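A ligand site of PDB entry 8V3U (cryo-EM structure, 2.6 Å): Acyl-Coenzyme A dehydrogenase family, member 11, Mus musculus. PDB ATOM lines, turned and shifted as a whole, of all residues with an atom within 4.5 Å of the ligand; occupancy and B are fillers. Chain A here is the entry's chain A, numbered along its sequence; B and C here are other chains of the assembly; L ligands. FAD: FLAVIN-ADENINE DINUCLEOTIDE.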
ATOM      1  N   PHE A 502      15.171   3.363   8.313  1.00  0.00           N
ATOM      2  CA  PHE A 502      15.439   4.727   7.868  1.00  0.00           C
ATOM      3  C   PHE A 502      16.649   4.705   6.951  1.00  0.00           C
ATOM      4  O   PHE A 502      17.716   4.240   7.347  1.00  0.00           O
ATOM      5  CB  PHE A 502      15.669   5.656   9.052  1.00  0.00           C
ATOM      6  CG  PHE A 502      16.041   7.056   8.669  1.00  0.00           C
ATOM      7  CD1 PHE A 502      15.118   7.882   8.047  1.00  0.00           C
ATOM      8  CD2 PHE A 502      17.306   7.550   8.928  1.00  0.00           C
ATOM      9  CE1 PHE A 502      15.457   9.176   7.691  1.00  0.00           C
ATOM     10  CE2 PHE A 502      17.648   8.838   8.580  1.00  0.00           C
ATOM     11  CZ  PHE A 502      16.723   9.651   7.962  1.00  0.00           C
ATOM     12  N   CYS A 503      16.488   5.204   5.725  1.00  0.00           N
ATOM     13  CA  CYS A 503      17.539   5.173   4.723  1.00  0.00           C
ATOM     14  C   CYS A 503      17.698   6.546   4.108  1.00  0.00           C
ATOM     15  O   CYS A 503      16.771   7.059   3.468  1.00  0.00           O
ATOM     16  CB  CYS A 503      17.261   4.129   3.645  1.00  0.00           C
ATOM     17  SG  CYS A 503      15.526   3.944   3.204  1.00  0.00           S
ATOM     18  N   MET A 504      18.869   7.162   4.299  1.00  0.00           N
ATOM     19  CA  MET A 504      19.174   8.438   3.671  1.00  0.00           C
ATOM     20  C   MET A 504      20.617   8.545   3.182  1.00  0.00           C
ATOM     21  O   MET A 504      20.994   9.602   2.664  1.00  0.00           O
ATOM     22  CB  MET A 504      18.888   9.586   4.652  1.00  0.00           C
ATOM     23  CG  MET A 504      19.982   9.819   5.678  1.00  0.00           C
ATOM     24  SD  MET A 504      20.133  11.561   6.131  1.00  0.00           S
ATOM     25  CE  MET A 504      21.585  12.018   5.190  1.00  0.00           C
ATOM     26  N   THR A 505      21.421   7.503   3.305  1.00  0.00           N
ATOM     27  CA  THR A 505      22.837   7.539   2.959  1.00  0.00           C
ATOM     28  C   THR A 505      23.057   6.879   1.604  1.00  0.00           C
ATOM     29  O   THR A 505      22.504   5.802   1.345  1.00  0.00           O
ATOM     30  CB  THR A 505      23.678   6.852   4.030  1.00  0.00           C
ATOM     31  OG1 THR A 505      23.593   7.606   5.254  1.00  0.00           O
ATOM     32  CG2 THR A 505      25.126   6.744   3.617  1.00  0.00           C
ATOM     33  N   VAL A 509      28.502   8.920  -2.806  1.00  0.00           N
ATOM     34  CA  VAL A 509      28.697  10.316  -2.480  1.00  0.00           C
ATOM     35  C   VAL A 509      29.006  10.438  -0.992  1.00  0.00           C
ATOM     36  O   VAL A 509      28.869   9.490  -0.232  1.00  0.00           O
ATOM     37  CB  VAL A 509      27.475  11.198  -2.847  1.00  0.00           C
ATOM     38  CG1 VAL A 509      27.171  11.099  -4.335  1.00  0.00           C
ATOM     39  CG2 VAL A 509      26.273  10.810  -2.012  1.00  0.00           C
ATOM     40  N   SER A 510      29.432  11.635  -0.593  1.00  0.00           N
ATOM     41  CA  SER A 510      29.678  11.946   0.811  1.00  0.00           C
ATOM     42  C   SER A 510      28.352  12.359   1.449  1.00  0.00           C
ATOM     43  O   SER A 510      27.873  13.479   1.223  1.00  0.00           O
ATOM     44  CB  SER A 510      30.729  13.042   0.945  1.00  0.00           C
ATOM     45  OG  SER A 510      32.023  12.549   0.668  1.00  0.00           O
ATOM     46  N   SER A 511      27.773  11.472   2.239  1.00  0.00           N
ATOM     47  CA  SER A 511      26.455  11.696   2.826  1.00  0.00           C
ATOM     48  C   SER A 511      26.502  12.404   4.172  1.00  0.00           C
ATOM     49  O   SER A 511      25.444  12.701   4.731  1.00  0.00           O
ATOM     50  CB  SER A 511      25.715  10.362   2.978  1.00  0.00           C
ATOM     51  OG  SER A 511      25.790   9.615   1.775  1.00  0.00           O
ATOM     52  N   SER A 512      27.689  12.685   4.711  1.00  0.00           N
ATOM     53  CA  SER A 512      27.768  13.505   5.903  1.00  0.00           C
ATOM     54  C   SER A 512      27.261  14.913   5.653  1.00  0.00           C
ATOM     55  O   SER A 512      26.827  15.587   6.596  1.00  0.00           O
ATOM     56  CB  SER A 512      29.198  13.535   6.434  1.00  0.00           C
ATOM     57  OG  SER A 512      30.104  13.998   5.448  1.00  0.00           O
ATOM     58  N   TRP A 535      22.166   2.828   1.360  1.00  0.00           N
ATOM     59  CA  TRP A 535      23.471   2.442   1.886  1.00  0.00           C
ATOM     60  C   TRP A 535      23.408   2.427   3.401  1.00  0.00           C
ATOM     61  O   TRP A 535      22.945   3.397   4.012  1.00  0.00           O
ATOM     62  CB  TRP A 535      24.524   3.424   1.362  1.00  0.00           C
ATOM     63  CG  TRP A 535      25.967   3.140   1.619  1.00  0.00           C
ATOM     64  CD1 TRP A 535      26.878   3.979   2.184  1.00  0.00           C
ATOM     65  CD2 TRP A 535      26.686   1.945   1.274  1.00  0.00           C
ATOM     66  NE1 TRP A 535      28.111   3.379   2.231  1.00  0.00           N
ATOM     67  CE2 TRP A 535      28.025   2.135   1.685  1.00  0.00           C
ATOM     68  CE3 TRP A 535      26.327   0.740   0.671  1.00  0.00           C
ATOM     69  CZ2 TRP A 535      29.004   1.162   1.512  1.00  0.00           C
ATOM     70  CZ3 TRP A 535      27.307  -0.220   0.495  1.00  0.00           C
ATOM     71  CH2 TRP A 535      28.622  -0.010   0.917  1.00  0.00           C
ATOM     72  N   TRP A 536      23.846   1.314   4.000  1.00  0.00           N
ATOM     73  CA  TRP A 536      23.934   1.169   5.462  1.00  0.00           C
ATOM     74  C   TRP A 536      22.563   1.234   6.125  1.00  0.00           C
ATOM     75  O   TRP A 536      22.425   1.703   7.254  1.00  0.00           O
ATOM     76  CB  TRP A 536      24.881   2.220   6.063  1.00  0.00           C
ATOM     77  CG  TRP A 536      26.318   1.844   5.942  1.00  0.00           C
ATOM     78  CD1 TRP A 536      27.239   2.378   5.093  1.00  0.00           C
ATOM     79  CD2 TRP A 536      27.015   0.855   6.708  1.00  0.00           C
ATOM     80  NE1 TRP A 536      28.457   1.779   5.277  1.00  0.00           N
ATOM     81  CE2 TRP A 536      28.348   0.837   6.265  1.00  0.00           C
ATOM     82  CE3 TRP A 536      26.636  -0.024   7.735  1.00  0.00           C
ATOM     83  CZ2 TRP A 536      29.301  -0.014   6.805  1.00  0.00           C
ATOM     84  CZ3 TRP A 536      27.594  -0.870   8.263  1.00  0.00           C
ATOM     85  CH2 TRP A 536      28.911  -0.857   7.798  1.00  0.00           C
ATOM     86  N   SER A 538      19.970   0.100   8.305  1.00  0.00           N
ATOM     87  CA  SER A 538      19.966  -0.830   9.427  1.00  0.00           C
ATOM     88  C   SER A 538      18.589  -1.454   9.615  1.00  0.00           C
ATOM     89  O   SER A 538      17.576  -0.745   9.636  1.00  0.00           O
ATOM     90  CB  SER A 538      20.392  -0.106  10.707  1.00  0.00           C
ATOM     91  OG  SER A 538      21.665   0.479  10.560  1.00  0.00           O
ATOM     92  N   VAL A 585      30.684  -5.139   9.813  1.00  0.00           N
ATOM     93  CA  VAL A 585      31.370  -4.194  10.678  1.00  0.00           C
ATOM     94  C   VAL A 585      32.517  -4.940  11.346  1.00  0.00           C
ATOM     95  O   VAL A 585      32.284  -5.747  12.248  1.00  0.00           O
ATOM     96  CB  VAL A 585      30.438  -3.562  11.718  1.00  0.00           C
ATOM     97  CG1 VAL A 585      31.236  -2.858  12.791  1.00  0.00           C
ATOM     98  CG2 VAL A 585      29.461  -2.611  11.053  1.00  0.00           C
ATOM     99  N   HIS A 596      22.887  -4.453   8.323  1.00  0.00           N
ATOM    100  CA  HIS A 596      22.954  -3.224   7.549  1.00  0.00           C
ATOM    101  C   HIS A 596      23.034  -3.588   6.077  1.00  0.00           C
ATOM    102  O   HIS A 596      23.850  -4.414   5.687  1.00  0.00           O
ATOM    103  CB  HIS A 596      24.156  -2.376   7.961  1.00  0.00           C
ATOM    104  CG  HIS A 596      24.402  -2.354   9.442  1.00  0.00           C
ATOM    105  ND1 HIS A 596      23.707  -1.519  10.298  1.00  0.00           N
ATOM    106  CD2 HIS A 596      25.251  -3.068  10.216  1.00  0.00           C
ATOM    107  CE1 HIS A 596      24.120  -1.723  11.532  1.00  0.00           C
ATOM    108  NE2 HIS A 596      25.057  -2.653  11.512  1.00  0.00           N
ATOM    109  N   THR A 747      31.831   2.171  15.606  1.00  0.00           N
ATOM    110  CA  THR A 747      30.889   2.665  14.605  1.00  0.00           C
ATOM    111  C   THR A 747      30.046   3.832  15.111  1.00  0.00           C
ATOM    112  O   THR A 747      29.370   4.470  14.302  1.00  0.00           O
ATOM    113  CB  THR A 747      29.968   1.544  14.138  1.00  0.00           C
ATOM    114  OG1 THR A 747      29.390   0.888  15.279  1.00  0.00           O
ATOM    115  CG2 THR A 747      30.741   0.550  13.318  1.00  0.00           C
ATOM    116  N   LEU A 750      30.840   7.321  13.602  1.00  0.00           N
ATOM    117  CA  LEU A 750      30.477   7.544  12.205  1.00  0.00           C
ATOM    118  C   LEU A 750      28.975   7.593  11.984  1.00  0.00           C
ATOM    119  O   LEU A 750      28.503   8.419  11.202  1.00  0.00           O
ATOM    120  CB  LEU A 750      31.084   6.460  11.321  1.00  0.00           C
ATOM    121  CG  LEU A 750      32.605   6.312  11.372  1.00  0.00           C
ATOM    122  CD1 LEU A 750      33.019   4.870  11.153  1.00  0.00           C
ATOM    123  CD2 LEU A 750      33.260   7.223  10.359  1.00  0.00           C
ATOM    124  N   ALA A 751      28.218   6.736  12.660  1.00  0.00           N
ATOM    125  CA  ALA A 751      26.764   6.725  12.505  1.00  0.00           C
ATOM    126  C   ALA A 751      26.150   7.984  13.102  1.00  0.00           C
ATOM    127  O   ALA A 751      26.654   8.548  14.077  1.00  0.00           O
ATOM    128  CB  ALA A 751      26.169   5.486  13.149  1.00  0.00           C
ATOM    129  N   ASP A 752      25.033   8.411  12.516  1.00  0.00           N
ATOM    130  CA  ASP A 752      24.341   9.638  12.913  1.00  0.00           C
ATOM    131  C   ASP A 752      25.255  10.863  12.819  1.00  0.00           C
ATOM    132  O   ASP A 752      25.195  11.772  13.638  1.00  0.00           O
ATOM    133  CB  ASP A 752      23.750   9.515  14.318  1.00  0.00           C
ATOM    134  CG  ASP A 752      22.533   8.614  14.368  1.00  0.00           C
ATOM    135  OD1 ASP A 752      21.579   8.870  13.603  1.00  0.00           O
ATOM    136  OD2 ASP A 752      22.532   7.649  15.165  1.00  0.00           O
ATOM    137  N   GLY A 753      26.116  10.866  11.803  1.00  0.00           N
ATOM    138  CA  GLY A 753      27.034  11.963  11.588  1.00  0.00           C
ATOM    139  C   GLY A 753      28.359  11.758  12.277  1.00  0.00           C
ATOM    140  O   GLY A 753      28.444  11.326  13.427  1.00  0.00           O
ATOM    141  N   PRO A 754      29.444  12.081  11.572  1.00  0.00           N
ATOM    142  CA  PRO A 754      30.782  11.985  12.179  1.00  0.00           C
ATOM    143  C   PRO A 754      30.984  13.039  13.244  1.00  0.00           C
ATOM    144  O   PRO A 754      30.181  13.958  13.436  1.00  0.00           O
ATOM    145  CB  PRO A 754      31.725  12.208  10.989  1.00  0.00           C
ATOM    146  CG  PRO A 754      30.895  11.968   9.772  1.00  0.00           C
ATOM    147  CD  PRO A 754      29.516  12.387  10.135  1.00  0.00           C
ATOM    148  N   GLU A 756      33.449  15.225  13.384  1.00  0.00           N
ATOM    149  CA  GLU A 756      34.029  16.470  12.894  1.00  0.00           C
ATOM    150  C   GLU A 756      32.954  17.490  12.541  1.00  0.00           C
ATOM    151  O   GLU A 756      33.102  18.696  12.825  1.00  0.00           O
ATOM    152  CB  GLU A 756      34.926  16.187  11.693  1.00  0.00           C
ATOM    153  CG  GLU A 756      36.284  15.617  12.063  1.00  0.00           C
ATOM    154  CD  GLU A 756      36.244  14.134  12.380  1.00  0.00           C
ATOM    155  OE1 GLU A 756      35.300  13.447  11.939  1.00  0.00           O
ATOM    156  OE2 GLU A 756      37.159  13.654  13.088  1.00  0.00           O
ATOM    157  N   VAL A 757      31.851  17.050  11.929  1.00  0.00           N
ATOM    158  CA  VAL A 757      30.768  17.975  11.600  1.00  0.00           C
ATOM    159  C   VAL A 757      30.131  18.512  12.880  1.00  0.00           C
ATOM    160  O   VAL A 757      29.773  19.686  12.958  1.00  0.00           O
ATOM    161  CB  VAL A 757      29.735  17.294  10.680  1.00  0.00           C
ATOM    162  CG1 VAL A 757      30.386  16.888   9.372  1.00  0.00           C
ATOM    163  CG2 VAL A 757      29.111  16.084  11.344  1.00  0.00           C
ATOM    164  N   SER A 760      32.431  21.177  14.260  1.00  0.00           N
ATOM    165  CA  SER A 760      32.250  22.422  13.521  1.00  0.00           C
ATOM    166  C   SER A 760      30.974  23.147  13.935  1.00  0.00           C
ATOM    167  O   SER A 760      30.968  24.367  14.111  1.00  0.00           O
ATOM    168  CB  SER A 760      32.251  22.139  12.023  1.00  0.00           C
ATOM    169  OG  SER A 760      33.481  21.578  11.604  1.00  0.00           O
ATOM    170  N   GLU B 666      40.196  25.036  10.499  1.00  0.00           N
ATOM    171  CA  GLU B 666      39.397  24.081  11.264  1.00  0.00           C
ATOM    172  C   GLU B 666      40.042  23.696  12.584  1.00  0.00           C
ATOM    173  O   GLU B 666      39.334  23.323  13.528  1.00  0.00           O
ATOM    174  CB  GLU B 666      39.137  22.833  10.421  1.00  0.00           C
ATOM    175  CG  GLU B 666      37.783  22.823   9.770  1.00  0.00           C
ATOM    176  CD  GLU B 666      37.228  21.431   9.595  1.00  0.00           C
ATOM    177  OE1 GLU B 666      36.066  21.312   9.175  1.00  0.00           O
ATOM    178  OE2 GLU B 666      37.961  20.463   9.891  1.00  0.00           O
ATOM    179  N   ARG C 655      37.189  12.483  -2.609  1.00  0.00           N
ATOM    180  CA  ARG C 655      35.859  12.818  -2.106  1.00  0.00           C
ATOM    181  C   ARG C 655      35.705  14.314  -1.851  1.00  0.00           C
ATOM    182  O   ARG C 655      36.676  15.035  -1.579  1.00  0.00           O
ATOM    183  CB  ARG C 655      35.567  12.040  -0.832  1.00  0.00           C
ATOM    184  CG  ARG C 655      35.652  10.536  -1.000  1.00  0.00           C
ATOM    185  CD  ARG C 655      34.403  10.002  -1.660  1.00  0.00           C
ATOM    186  NE  ARG C 655      33.351   9.733  -0.680  1.00  0.00           N
ATOM    187  CZ  ARG C 655      32.411   8.813  -0.837  1.00  0.00           C
ATOM    188  NH1 ARG C 655      32.354   8.064  -1.921  1.00  0.00           N
ATOM    189  NH2 ARG C 655      31.514   8.644   0.126  1.00  0.00           N
ATOM    190  N   ALA C 657      33.055  17.091   0.286  1.00  0.00           N
ATOM    191  CA  ALA C 657      31.988  17.284   1.256  1.00  0.00           C
ATOM    192  C   ALA C 657      31.957  18.744   1.696  1.00  0.00           C
ATOM    193  O   ALA C 657      33.011  19.348   1.913  1.00  0.00           O
ATOM    194  CB  ALA C 657      32.167  16.378   2.478  1.00  0.00           C
ATOM    195  N   PHE C 658      30.753  19.291   1.820  1.00  0.00           N
ATOM    196  CA  PHE C 658      30.540  20.684   2.219  1.00  0.00           C
ATOM    197  C   PHE C 658      31.252  21.647   1.261  1.00  0.00           C
ATOM    198  O   PHE C 658      31.962  22.560   1.675  1.00  0.00           O
ATOM    199  CB  PHE C 658      30.978  20.907   3.664  1.00  0.00           C
ATOM    200  CG  PHE C 658      30.138  20.173   4.673  1.00  0.00           C
ATOM    201  CD1 PHE C 658      28.960  20.715   5.147  1.00  0.00           C
ATOM    202  CD2 PHE C 658      30.529  18.928   5.142  1.00  0.00           C
ATOM    203  CE1 PHE C 658      28.189  20.040   6.066  1.00  0.00           C
ATOM    204  CE2 PHE C 658      29.765  18.250   6.057  1.00  0.00           C
ATOM    205  CZ  PHE C 658      28.589  18.806   6.528  1.00  0.00           C
ATOM    206  N   LEU C 662      37.980  16.609   0.770  1.00  0.00           N
ATOM    207  CA  LEU C 662      38.268  16.208   2.133  1.00  0.00           C
ATOM    208  C   LEU C 662      39.600  16.758   2.627  1.00  0.00           C
ATOM    209  O   LEU C 662      39.723  17.161   3.783  1.00  0.00           O
ATOM    210  CB  LEU C 662      38.235  14.681   2.258  1.00  0.00           C
ATOM    211  CG  LEU C 662      36.890  13.984   2.066  1.00  0.00           C
ATOM    212  CD1 LEU C 662      36.973  12.540   2.517  1.00  0.00           C
ATOM    213  CD2 LEU C 662      35.779  14.720   2.798  1.00  0.00           C
ATOM    214  N   HIS C 665      39.836  20.336   4.150  1.00  0.00           N
ATOM    215  CA  HIS C 665      39.634  20.487   5.583  1.00  0.00           C
ATOM    216  C   HIS C 665      40.963  20.243   6.294  1.00  0.00           C
ATOM    217  O   HIS C 665      41.657  19.261   6.023  1.00  0.00           O
ATOM    218  CB  HIS C 665      38.570  19.508   6.087  1.00  0.00           C
ATOM    219  CG  HIS C 665      37.215  19.742   5.496  1.00  0.00           C
ATOM    220  ND1 HIS C 665      36.627  18.883   4.602  1.00  0.00           N
ATOM    221  CD2 HIS C 665      36.324  20.748   5.684  1.00  0.00           C
ATOM    222  CE1 HIS C 665      35.436  19.336   4.261  1.00  0.00           C
ATOM    223  NE2 HIS C 665      35.233  20.476   4.902  1.00  0.00           N
ATOM    224  N   GLN C 725      38.473   6.565   9.709  1.00  0.00           N
ATOM    225  CA  GLN C 725      37.599   7.719   9.906  1.00  0.00           C
ATOM    226  C   GLN C 725      37.459   8.533   8.627  1.00  0.00           C
ATOM    227  O   GLN C 725      36.384   9.062   8.332  1.00  0.00           O
ATOM    228  CB  GLN C 725      38.120   8.589  11.045  1.00  0.00           C
ATOM    229  CG  GLN C 725      37.154   9.659  11.504  1.00  0.00           C
ATOM    230  CD  GLN C 725      35.923   9.096  12.199  1.00  0.00           C
ATOM    231  OE1 GLN C 725      35.993   8.057  12.846  1.00  0.00           O
ATOM    232  NE2 GLN C 725      34.801   9.781  12.064  1.00  0.00           N
ATOM    233  N   VAL C 726      38.544   8.663   7.859  1.00  0.00           N
ATOM    234  CA  VAL C 726      38.496   9.402   6.605  1.00  0.00           C
ATOM    235  C   VAL C 726      37.555   8.733   5.616  1.00  0.00           C
ATOM    236  O   VAL C 726      36.769   9.392   4.933  1.00  0.00           O
ATOM    237  CB  VAL C 726      39.911   9.574   6.020  1.00  0.00           C
ATOM    238  CG1 VAL C 726      39.852   9.887   4.538  1.00  0.00           C
ATOM    239  CG2 VAL C 726      40.672  10.642   6.761  1.00  0.00           C
ATOM    240  N   HIS C 727      37.604   7.402   5.538  1.00  0.00           N
ATOM    241  CA  HIS C 727      36.745   6.711   4.577  1.00  0.00           C
ATOM    242  C   HIS C 727      35.276   6.728   4.971  1.00  0.00           C
ATOM    243  O   HIS C 727      34.418   6.435   4.131  1.00  0.00           O
ATOM    244  CB  HIS C 727      37.222   5.270   4.385  1.00  0.00           C
ATOM    245  CG  HIS C 727      38.300   5.131   3.372  1.00  0.00           C
ATOM    246  ND1 HIS C 727      38.097   4.505   2.151  1.00  0.00           N
ATOM    247  CD2 HIS C 727      39.590   5.533   3.370  1.00  0.00           C
ATOM    248  CE1 HIS C 727      39.219   4.533   1.449  1.00  0.00           C
ATOM    249  NE2 HIS C 727      40.145   5.148   2.171  1.00  0.00           N
ATOM    250  N   GLY C 728      34.948   7.054   6.217  1.00  0.00           N
ATOM    251  CA  GLY C 728      33.571   7.131   6.643  1.00  0.00           C
ATOM    252  C   GLY C 728      32.983   5.789   7.039  1.00  0.00           C
ATOM    253  O   GLY C 728      33.667   4.951   7.620  1.00  0.00           O
ATOM    254  N   GLY C 729      31.697   5.583   6.725  1.00  0.00           N
ATOM    255  CA  GLY C 729      31.068   4.318   7.038  1.00  0.00           C
ATOM    256  C   GLY C 729      31.679   3.147   6.298  1.00  0.00           C
ATOM    257  O   GLY C 729      31.716   2.027   6.821  1.00  0.00           O
ATOM    258  N   VAL C 732      34.692   0.662   7.773  1.00  0.00           N
ATOM    259  CA  VAL C 732      34.539  -0.546   8.572  1.00  0.00           C
ATOM    260  C   VAL C 732      33.977  -1.713   7.767  1.00  0.00           C
ATOM    261  O   VAL C 732      33.946  -2.839   8.276  1.00  0.00           O
ATOM    262  CB  VAL C 732      33.641  -0.292   9.804  1.00  0.00           C
ATOM    263  CG1 VAL C 732      34.202   0.847  10.640  1.00  0.00           C
ATOM    264  CG2 VAL C 732      32.207  -0.001   9.379  1.00  0.00           C
HETATM  265  PA  FAD L   1      31.775  10.582   4.304  1.00  0.00           P
HETATM  266  O1A FAD L   1      31.989   9.908   3.006  1.00  0.00           O
HETATM  267  O2A FAD L   1      31.211  12.001   4.214  1.00  0.00           O
HETATM  268  O5B FAD L   1      33.084  10.585   5.164  1.00  0.00           O
HETATM  269  C5B FAD L   1      34.137  11.541   4.934  1.00  0.00           C
HETATM  270  C4B FAD L   1      34.877  11.798   6.214  1.00  0.00           C
HETATM  271  O4B FAD L   1      35.455  13.111   6.178  1.00  0.00           O
HETATM  272  C3B FAD L   1      34.012  11.771   7.475  1.00  0.00           C
HETATM  273  O3B FAD L   1      33.905  10.456   7.994  1.00  0.00           O
HETATM  274  C2B FAD L   1      34.796  12.685   8.420  1.00  0.00           C
HETATM  275  O2B FAD L   1      35.831  11.995   9.096  1.00  0.00           O
HETATM  276  C1B FAD L   1      35.378  13.723   7.452  1.00  0.00           C
HETATM  277  N9A FAD L   1      34.601  14.943   7.344  1.00  0.00           N
HETATM  278  C8A FAD L   1      33.378  15.111   6.743  1.00  0.00           C
HETATM  279  N7A FAD L   1      32.909  16.332   6.796  1.00  0.00           N
HETATM  280  C5A FAD L   1      33.886  17.018   7.496  1.00  0.00           C
HETATM  281  C6A FAD L   1      33.991  18.366   7.890  1.00  0.00           C
HETATM  282  N6A FAD L   1      33.059  19.297   7.634  1.00  0.00           N
HETATM  283  N1A FAD L   1      35.099  18.738   8.580  1.00  0.00           N
HETATM  284  C2A FAD L   1      36.024  17.823   8.837  1.00  0.00           C
HETATM  285  N3A FAD L   1      36.041  16.525   8.508  1.00  0.00           N
HETATM  286  C4A FAD L   1      34.929  16.182   7.840  1.00  0.00           C
HETATM  287  N1  FAD L   1      22.957   5.665   7.489  1.00  0.00           N
HETATM  288  C2  FAD L   1      21.601   5.754   7.380  1.00  0.00           C
HETATM  289  O2  FAD L   1      21.057   6.552   6.608  1.00  0.00           O
HETATM  290  N3  FAD L   1      20.791   4.940   8.149  1.00  0.00           N
HETATM  291  C4  FAD L   1      21.221   4.006   9.064  1.00  0.00           C
HETATM  292  O4  FAD L   1      20.402   3.340   9.697  1.00  0.00           O
HETATM  293  C4X FAD L   1      22.660   3.924   9.170  1.00  0.00           C
HETATM  294  N5  FAD L   1      23.166   3.051  10.008  1.00  0.00           N
HETATM  295  C5X FAD L   1      24.544   2.966  10.112  1.00  0.00           C
HETATM  296  C6  FAD L   1      25.092   2.044  11.001  1.00  0.00           C
HETATM  297  C7  FAD L   1      26.468   1.918  11.139  1.00  0.00           C
HETATM  298  C7M FAD L   1      27.025   0.922  12.114  1.00  0.00           C
HETATM  299  C8  FAD L   1      27.315   2.736  10.371  1.00  0.00           C
HETATM  300  C8M FAD L   1      28.817   2.625  10.495  1.00  0.00           C
HETATM  301  C9  FAD L   1      26.771   3.648   9.473  1.00  0.00           C
HETATM  302  C9A FAD L   1      25.390   3.771   9.347  1.00  0.00           C
HETATM  303  N10 FAD L   1      24.809   4.697   8.461  1.00  0.00           N
HETATM  304  C10 FAD L   1      23.442   4.788   8.333  1.00  0.00           C
HETATM  305  C1' FAD L   1      25.645   5.561   7.615  1.00  0.00           C
HETATM  306  C2' FAD L   1      26.183   6.787   8.354  1.00  0.00           C
HETATM  307  O2' FAD L   1      25.129   7.718   8.618  1.00  0.00           O
HETATM  308  C3' FAD L   1      27.249   7.460   7.495  1.00  0.00           C
HETATM  309  O3' FAD L   1      28.357   6.568   7.367  1.00  0.00           O
HETATM  310  C4' FAD L   1      27.752   8.796   8.029  1.00  0.00           C
HETATM  311  O4' FAD L   1      26.645   9.678   8.201  1.00  0.00           O
HETATM  312  C5' FAD L   1      28.798   9.425   7.132  1.00  0.00           C
HETATM  313  O5' FAD L   1      28.462   9.146   5.762  1.00  0.00           O
HETATM  314  P   FAD L   1      29.575   8.856   4.690  1.00  0.00           P
HETATM  315  O1P FAD L   1      29.983   7.384   4.778  1.00  0.00           O
HETATM  316  O2P FAD L   1      29.165   9.306   3.360  1.00  0.00           O
HETATM  317  O3P FAD L   1      30.787   9.731   5.209  1.00  0.00           O
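The side-chain hydroxyl (OG) of Ser 512 is in hydrogen-bond range of an oxygen (O2A) of the ligand, 2.6 Å away. N of Ser 511 is in hydrogen-bond range of O2P of the ligand (2.8 Å). N1A of the ligand is in hydrogen-bond range of OE1 of Glu 666 of chain B (2.8 Å). The backbone carbonyl oxygen (O) of Gln 725 of chain C lies within hydrogen-bond range of an oxygen (O3B) of the ligand, 2.9 Å away. The backbone NH (N) of Thr 505 lies within hydrogen-bond range of an oxygen (O2) of the ligand (3.5 Å). The side-chain hydroxyl (OG1) of Thr 505 sits at hydrogen-bond distance from a nitrogen (N1) of the ligand. The side-chain hydroxyl (OG) of Ser 538 is in hydrogen-bond range of a nitrogen (N5) of the ligand. The backbone NH of Gly 729 of chain C sits at hydrogen-bond distance from an oxygen (O1P) of the ligand. O1A of the ligand lies within salt-bridge range of NH2 of Arg 655 of chain C, 3.2 Å away. O2B of the ligand is in hydrogen-bond range of OE1 of Glu 756. The backbone NH (N) of Met 504 is in hydrogen-bond range of an oxygen (O2) of the ligand (3.2 Å). The backbone carbonyl oxygen of Phe 502 is in hydrogen-bond range of a nitrogen (N3) of the ligand.
The backbone NH (N) of Trp 535 sits at hydrogen-bond distance from the backbone carbonyl oxygen (O) of Thr 505, 3.0 Å away. The side-chain hydroxyl (OG) of Ser 538 is in hydrogen-bond range of a ring nitrogen (ND1) of His 596, 2.9 Å away. The guanidinium group (NE) of Arg 655 of chain C sits at hydrogen-bond distance from the side-chain hydroxyl (OG) of Ser 510. O of Val 509 is in hydrogen-bond range of NH2 of Arg 655 of chain C. N of Leu 662 of chain C sits at hydrogen-bond distance from O of Arg 655 of chain C, at 3.1 Å. OG of Ser 760 is in hydrogen-bond range of O of Glu 756, 3.2 Å away.
The backbone carbonyl oxygen (O) of Trp 536 lies close to a nitrogen (N5) of the ligand (3.2 Å). Val 509 touches the ligand (O to O2P, 3.6 Å). Ser 510 touches the ligand. His 596 touches the ligand (ND1 to C6, 3.9 Å). Thr 747 touches the ligand. O of Leu 750 touches C4' of the ligand, 3.3 Å away. N of Asp 752 touches O2' of the ligand, 3.96 Å away. Gly 753 touches the ligand. Pro 754 touches the ligand. Val 757 touches the ligand (CG1 to N7A, 3.6 Å). CD2 of Phe 658 of chain C touches N6A of the ligand, at 3.6 Å. Leu 662 of chain C touches the ligand (CD2 to O4B, 3.8 Å). His 665 of chain C touches the ligand (NE2 to N6A, 3.7 Å). Val 726 of chain C touches the ligand (O to C4B, 3.3 Å). CA of Gly 728 of chain C touches O3B of the ligand, at 3.6 Å. Hydrophobic or aromatic side chains that line the ligand: Met 504, Trp 536, His 596, Pro 754, Val 757, Phe 658 of chain C, Leu 662 of chain C and His 665 of chain C. Within 4 Å of the ligand: Phe 502, Met 504, Thr 505, Val 509, Ser 510, Ser 511, Ser 512, Trp 536, Ser 538, His 596, Thr 747, Leu 750, Asp 752, Gly 753, Pro 754, Glu 756, Val 757, Glu 666 of chain B, Arg 655 of chain C, Phe 658 of chain C, Leu 662 of chain C, His 665 of chain C, Gln 725 of chain C, Val 726 of chain C, Gly 728 of chain C and Gly 729 of chain C.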
